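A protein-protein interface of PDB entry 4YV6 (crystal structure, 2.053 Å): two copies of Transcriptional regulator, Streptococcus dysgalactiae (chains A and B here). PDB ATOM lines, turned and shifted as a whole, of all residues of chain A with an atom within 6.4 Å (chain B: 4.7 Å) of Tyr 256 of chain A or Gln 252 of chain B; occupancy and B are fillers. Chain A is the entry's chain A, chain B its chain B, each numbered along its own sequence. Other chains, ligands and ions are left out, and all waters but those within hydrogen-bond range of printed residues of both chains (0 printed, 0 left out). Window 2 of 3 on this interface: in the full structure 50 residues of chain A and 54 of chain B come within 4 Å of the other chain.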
ATOM      1  N   LEU A 251      14.912  20.227   2.035  1.00  0.00           N
ATOM      2  CA  LEU A 251      15.956  21.033   2.661  1.00  0.00           C
ATOM      3  C   LEU A 251      15.360  22.122   3.544  1.00  0.00           C
ATOM      4  O   LEU A 251      15.915  22.459   4.589  1.00  0.00           O
ATOM      5  CB  LEU A 251      16.858  21.666   1.599  1.00  0.00           C
ATOM      6  CG  LEU A 251      17.659  20.703   0.721  1.00  0.00           C
ATOM      7  CD1 LEU A 251      18.387  21.472  -0.372  1.00  0.00           C
ATOM      8  CD2 LEU A 251      18.645  19.889   1.551  1.00  0.00           C
ATOM      9  N   GLN A 252      14.230  22.678   3.113  1.00  0.00           N
ATOM     10  CA  GLN A 252      13.552  23.715   3.881  1.00  0.00           C
ATOM     11  C   GLN A 252      13.000  23.146   5.184  1.00  0.00           C
ATOM     12  O   GLN A 252      13.037  23.810   6.219  1.00  0.00           O
ATOM     13  CB  GLN A 252      12.423  24.348   3.062  1.00  0.00           C
ATOM     14  CG  GLN A 252      12.898  25.219   1.907  1.00  0.00           C
ATOM     15  CD  GLN A 252      13.744  26.393   2.367  1.00  0.00           C
ATOM     16  OE1 GLN A 252      14.964  26.280   2.500  1.00  0.00           O
ATOM     17  NE2 GLN A 252      13.100  27.529   2.609  1.00  0.00           N
ATOM     18  N   ILE A 253      12.486  21.920   5.130  1.00  0.00           N
ATOM     19  CA  ILE A 253      11.990  21.249   6.328  1.00  0.00           C
ATOM     20  C   ILE A 253      13.110  21.103   7.354  1.00  0.00           C
ATOM     21  O   ILE A 253      12.912  21.378   8.537  1.00  0.00           O
ATOM     22  CB  ILE A 253      11.406  19.860   6.004  1.00  0.00           C
ATOM     23  CG1 ILE A 253      10.148  20.008   5.143  1.00  0.00           C
ATOM     24  CG2 ILE A 253      11.065  19.103   7.292  1.00  0.00           C
ATOM     25  CD1 ILE A 253       9.612  18.702   4.595  1.00  0.00           C
ATOM     26  N   PHE A 254      14.279  20.663   6.899  1.00  0.00           N
ATOM     27  CA  PHE A 254      15.439  20.525   7.779  1.00  0.00           C
ATOM     28  C   PHE A 254      15.791  21.869   8.408  1.00  0.00           C
ATOM     29  O   PHE A 254      16.035  21.958   9.610  1.00  0.00           O
ATOM     30  CB  PHE A 254      16.650  19.979   7.014  1.00  0.00           C
ATOM     31  CG  PHE A 254      16.512  18.544   6.576  1.00  0.00           C
ATOM     32  CD1 PHE A 254      15.893  17.607   7.385  1.00  0.00           C
ATOM     33  CD2 PHE A 254      17.017  18.131   5.353  1.00  0.00           C
ATOM     34  CE1 PHE A 254      15.774  16.287   6.979  1.00  0.00           C
ATOM     35  CE2 PHE A 254      16.901  16.816   4.944  1.00  0.00           C
ATOM     36  CZ  PHE A 254      16.276  15.894   5.758  1.00  0.00           C
ATOM     37  N   LYS A 255      15.812  22.912   7.584  1.00  0.00           N
ATOM     38  CA  LYS A 255      16.140  24.257   8.043  1.00  0.00           C
ATOM     39  C   LYS A 255      15.125  24.775   9.058  1.00  0.00           C
ATOM     40  O   LYS A 255      15.500  25.346  10.082  1.00  0.00           O
ATOM     41  CB  LYS A 255      16.222  25.214   6.851  1.00  0.00           C
ATOM     42  CG  LYS A 255      16.488  26.665   7.227  1.00  0.00           C
ATOM     43  CD  LYS A 255      16.580  27.545   5.993  1.00  0.00           C
ATOM     44  CE  LYS A 255      16.584  29.021   6.359  1.00  0.00           C
ATOM     45  NZ  LYS A 255      16.559  29.893   5.152  1.00  0.00           N
ATOM     46  N   TYR A 256      13.841  24.583   8.769  1.00  0.00           N
ATOM     47  CA  TYR A 256      12.779  25.071   9.645  1.00  0.00           C
ATOM     48  C   TYR A 256      12.807  24.378  11.005  1.00  0.00           C
ATOM     49  O   TYR A 256      12.478  24.988  12.022  1.00  0.00           O
ATOM     50  CB  TYR A 256      11.404  24.871   8.993  1.00  0.00           C
ATOM     51  CG  TYR A 256      11.158  25.704   7.749  1.00  0.00           C
ATOM     52  CD1 TYR A 256      12.007  26.746   7.398  1.00  0.00           C
ATOM     53  CD2 TYR A 256      10.067  25.448   6.929  1.00  0.00           C
ATOM     54  CE1 TYR A 256      11.777  27.506   6.264  1.00  0.00           C
ATOM     55  CE2 TYR A 256       9.830  26.204   5.795  1.00  0.00           C
ATOM     56  CZ  TYR A 256      10.688  27.229   5.467  1.00  0.00           C
ATOM     57  OH  TYR A 256      10.455  27.982   4.339  1.00  0.00           O
ATOM     58  N   LEU A 257      13.201  23.108  11.019  1.00  0.00           N
ATOM     59  CA  LEU A 257      13.233  22.326  12.252  1.00  0.00           C
ATOM     60  C   LEU A 257      14.570  22.465  12.980  1.00  0.00           C
ATOM     61  O   LEU A 257      14.782  21.853  14.026  1.00  0.00           O
ATOM     62  CB  LEU A 257      12.957  20.850  11.955  1.00  0.00           C
ATOM     63  CG  LEU A 257      11.590  20.528  11.342  1.00  0.00           C
ATOM     64  CD1 LEU A 257      11.518  19.056  10.965  1.00  0.00           C
ATOM     65  CD2 LEU A 257      10.455  20.890  12.288  1.00  0.00           C
ATOM     66  N   GLY A 258      15.470  23.268  12.423  1.00  0.00           N
ATOM     67  CA  GLY A 258      16.764  23.505  13.040  1.00  0.00           C
ATOM     68  C   GLY A 258      17.680  22.295  12.992  1.00  0.00           C
ATOM     69  O   GLY A 258      18.579  22.157  13.823  1.00  0.00           O
ATOM     70  N   GLU A 259      17.452  21.418  12.019  1.00  0.00           N
ATOM     71  CA  GLU A 259      18.276  20.226  11.842  1.00  0.00           C
ATOM     72  C   GLU A 259      19.475  20.539  10.954  1.00  0.00           C
ATOM     73  O   GLU A 259      19.497  20.187   9.775  1.00  0.00           O
ATOM     74  CB  GLU A 259      17.449  19.092  11.237  1.00  0.00           C
ATOM     75  CG  GLU A 259      16.284  18.656  12.109  1.00  0.00           C
ATOM     76  CD  GLU A 259      16.729  18.000  13.404  1.00  0.00           C
ATOM     77  OE1 GLU A 259      17.804  17.362  13.417  1.00  0.00           O
ATOM     78  OE2 GLU A 259      16.002  18.125  14.412  1.00  0.00           O
ATOM     79  N   LEU B 228       6.964  23.352  16.703  1.00  0.00           N
ATOM     80  CA  LEU B 228       7.358  24.563  15.989  1.00  0.00           C
ATOM     81  C   LEU B 228       6.155  25.489  15.831  1.00  0.00           C
ATOM     82  O   LEU B 228       6.282  26.711  15.918  1.00  0.00           O
ATOM     83  CB  LEU B 228       7.950  24.219  14.619  1.00  0.00           C
ATOM     84  CG  LEU B 228       8.265  25.397  13.692  1.00  0.00           C
ATOM     85  CD1 LEU B 228       9.331  26.290  14.300  1.00  0.00           C
ATOM     86  CD2 LEU B 228       8.698  24.894  12.324  1.00  0.00           C
ATOM     87  N   ARG B 248       3.846  29.542  10.100  1.00  0.00           N
ATOM     88  CA  ARG B 248       3.741  29.399   8.652  1.00  0.00           C
ATOM     89  C   ARG B 248       4.741  28.376   8.123  1.00  0.00           C
ATOM     90  O   ARG B 248       4.466  27.674   7.151  1.00  0.00           O
ATOM     91  CB  ARG B 248       3.951  30.745   7.963  1.00  0.00           C
ATOM     92  CG  ARG B 248       2.664  31.516   7.727  1.00  0.00           C
ATOM     93  CD  ARG B 248       2.943  32.882   7.130  1.00  0.00           C
ATOM     94  NE  ARG B 248       3.641  33.750   8.074  1.00  0.00           N
ATOM     95  CZ  ARG B 248       4.192  34.917   7.755  1.00  0.00           C
ATOM     96  NH1 ARG B 248       4.139  35.366   6.506  1.00  0.00           N
ATOM     97  NH2 ARG B 248       4.803  35.635   8.687  1.00  0.00           N
ATOM     98  N   GLN B 249       5.904  28.297   8.763  1.00  0.00           N
ATOM     99  CA  GLN B 249       6.900  27.296   8.405  1.00  0.00           C
ATOM    100  C   GLN B 249       6.357  25.899   8.678  1.00  0.00           C
ATOM    101  O   GLN B 249       6.507  24.995   7.859  1.00  0.00           O
ATOM    102  CB  GLN B 249       8.204  27.521   9.178  1.00  0.00           C
ATOM    103  CG  GLN B 249       9.065  28.647   8.622  1.00  0.00           C
ATOM    104  CD  GLN B 249      10.233  28.997   9.523  1.00  0.00           C
ATOM    105  OE1 GLN B 249      10.562  28.258  10.449  1.00  0.00           O
ATOM    106  NE2 GLN B 249      10.866  30.133   9.253  1.00  0.00           N
ATOM    107  N   ALA B 250       5.715  25.737   9.830  1.00  0.00           N
ATOM    108  CA  ALA B 250       5.154  24.450  10.221  1.00  0.00           C
ATOM    109  C   ALA B 250       4.068  24.018   9.242  1.00  0.00           C
ATOM    110  O   ALA B 250       3.926  22.831   8.947  1.00  0.00           O
ATOM    111  CB  ALA B 250       4.598  24.521  11.635  1.00  0.00           C
ATOM    112  N   LEU B 251       3.305  24.984   8.740  1.00  0.00           N
ATOM    113  CA  LEU B 251       2.259  24.699   7.766  1.00  0.00           C
ATOM    114  C   LEU B 251       2.859  24.196   6.459  1.00  0.00           C
ATOM    115  O   LEU B 251       2.312  23.299   5.820  1.00  0.00           O
ATOM    116  CB  LEU B 251       1.407  25.945   7.506  1.00  0.00           C
ATOM    117  CG  LEU B 251       0.497  26.385   8.654  1.00  0.00           C
ATOM    118  CD1 LEU B 251      -0.151  27.720   8.336  1.00  0.00           C
ATOM    119  CD2 LEU B 251      -0.564  25.334   8.945  1.00  0.00           C
ATOM    120  N   GLN B 252       3.987  24.778   6.065  1.00  0.00           N
ATOM    121  CA  GLN B 252       4.666  24.371   4.842  1.00  0.00           C
ATOM    122  C   GLN B 252       5.192  22.943   4.948  1.00  0.00           C
ATOM    123  O   GLN B 252       5.167  22.195   3.970  1.00  0.00           O
ATOM    124  CB  GLN B 252       5.814  25.329   4.520  1.00  0.00           C
ATOM    125  CG  GLN B 252       5.360  26.731   4.151  1.00  0.00           C
ATOM    126  CD  GLN B 252       5.906  27.188   2.811  1.00  0.00           C
ATOM    127  OE1 GLN B 252       5.207  27.149   1.797  1.00  0.00           O
ATOM    128  NE2 GLN B 252       7.160  27.627   2.802  1.00  0.00           N
ATOM    129  N   ILE B 253       5.670  22.571   6.133  1.00  0.00           N
ATOM    130  CA  ILE B 253       6.162  21.213   6.361  1.00  0.00           C
ATOM    131  C   ILE B 253       5.045  20.200   6.113  1.00  0.00           C
ATOM    132  O   ILE B 253       5.214  19.263   5.334  1.00  0.00           O
ATOM    133  CB  ILE B 253       6.714  21.038   7.788  1.00  0.00           C
ATOM    134  CG1 ILE B 253       7.933  21.939   7.991  1.00  0.00           C
ATOM    135  CG2 ILE B 253       7.107  19.578   8.041  1.00  0.00           C
ATOM    136  CD1 ILE B 253       8.437  21.991   9.423  1.00  0.00           C
ATOM    137  N   PHE B 254       3.910  20.390   6.782  1.00  0.00           N
ATOM    138  CA  PHE B 254       2.734  19.549   6.557  1.00  0.00           C
ATOM    139  C   PHE B 254       2.410  19.464   5.070  1.00  0.00           C
ATOM    140  O   PHE B 254       2.116  18.389   4.548  1.00  0.00           O
ATOM    141  CB  PHE B 254       1.514  20.095   7.310  1.00  0.00           C
ATOM    142  CG  PHE B 254       1.612  19.988   8.807  1.00  0.00           C
ATOM    143  CD1 PHE B 254       2.108  18.843   9.411  1.00  0.00           C
ATOM    144  CD2 PHE B 254       1.197  21.036   9.610  1.00  0.00           C
ATOM    145  CE1 PHE B 254       2.192  18.751  10.787  1.00  0.00           C
ATOM    146  CE2 PHE B 254       1.280  20.950  10.987  1.00  0.00           C
ATOM    147  CZ  PHE B 254       1.777  19.805  11.576  1.00  0.00           C
ATOM    148  N   LYS B 255       2.470  20.607   4.394  1.00  0.00           N
ATOM    149  CA  LYS B 255       2.129  20.675   2.980  1.00  0.00           C
ATOM    150  C   LYS B 255       3.128  19.916   2.115  1.00  0.00           C
ATOM    151  O   LYS B 255       2.737  19.114   1.269  1.00  0.00           O
ATOM    152  CB  LYS B 255       2.054  22.129   2.519  1.00  0.00           C
ATOM    153  CG  LYS B 255       1.455  22.290   1.131  1.00  0.00           C
ATOM    154  CD  LYS B 255       1.220  23.752   0.778  1.00  0.00           C
ATOM    155  CE  LYS B 255       2.526  24.502   0.563  1.00  0.00           C
ATOM    156  NZ  LYS B 255       3.298  23.956  -0.589  1.00  0.00           N
ATOM    157  N   TYR B 256       4.415  20.177   2.326  1.00  0.00           N
ATOM    158  CA  TYR B 256       5.463  19.537   1.539  1.00  0.00           C
ATOM    159  C   TYR B 256       5.427  18.021   1.709  1.00  0.00           C
ATOM    160  O   TYR B 256       5.696  17.282   0.763  1.00  0.00           O
ATOM    161  CB  TYR B 256       6.844  20.080   1.931  1.00  0.00           C
ATOM    162  CG  TYR B 256       7.065  21.548   1.615  1.00  0.00           C
ATOM    163  CD1 TYR B 256       6.212  22.236   0.757  1.00  0.00           C
ATOM    164  CD2 TYR B 256       8.131  22.248   2.169  1.00  0.00           C
ATOM    165  CE1 TYR B 256       6.410  23.573   0.467  1.00  0.00           C
ATOM    166  CE2 TYR B 256       8.337  23.589   1.883  1.00  0.00           C
ATOM    167  CZ  TYR B 256       7.472  24.244   1.030  1.00  0.00           C
ATOM    168  OH  TYR B 256       7.668  25.576   0.737  1.00  0.00           O
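Among the printed residues, pairs that only touch across the chains: Tyr 256 of chain A with Gln 249 of chain B, Tyr 256 of chain A with Gln 252 of chain B, Leu 257 of chain A with Ile 253 of chain B and Tyr 256 of chain A with Leu 228 of chain B.
Along chain A the printed residues that touch a printed residue of chain B span positions 256 to 257. Of the 10 printed residues of chain B, 4 touch a printed residue of chain A. Printed residues of chain B that touch a printed residue of chain A: Leu 228, Gln 249, Gln 252 and Ile 253.
Ile 253 of chain A touches none of the printed residues of chain B. Tyr 256 of chain A touches just these residues of chain B: Leu 228, Gln 249 and Gln 252. Of the printed residues of chain B, Leu 257 of chain A touches Ile 253. Printed residues of chain A within 4 Å of Leu 228 of chain B: Tyr 256. Gln 252 of chain B touches just one residue of chain A: Tyr 256. Phe 254 of chain B touches none of the printed residues of chain A. The nearest residue of chain A that does not touch Gln 252 of chain B is Ile 253 of chain A (5.6 Å).
The side-chain hydroxyl (OH) of Tyr 256 of chain B sits at hydrogen-bond distance from the side-chain amide nitrogen (NE2) of Gln 252 of chain B (3.0 Å). The side-chain amide nitrogen (NE2) of Gln 252 of chain A sits at hydrogen-bond distance from the side-chain hydroxyl (OH) of Tyr 256 of chain A.
Tyr 256 of chain A touches Gln 252 of chain B, but with the chains exchanged Gln 252 of chain A does not touch Tyr 256 of chain B (4.3 Å).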
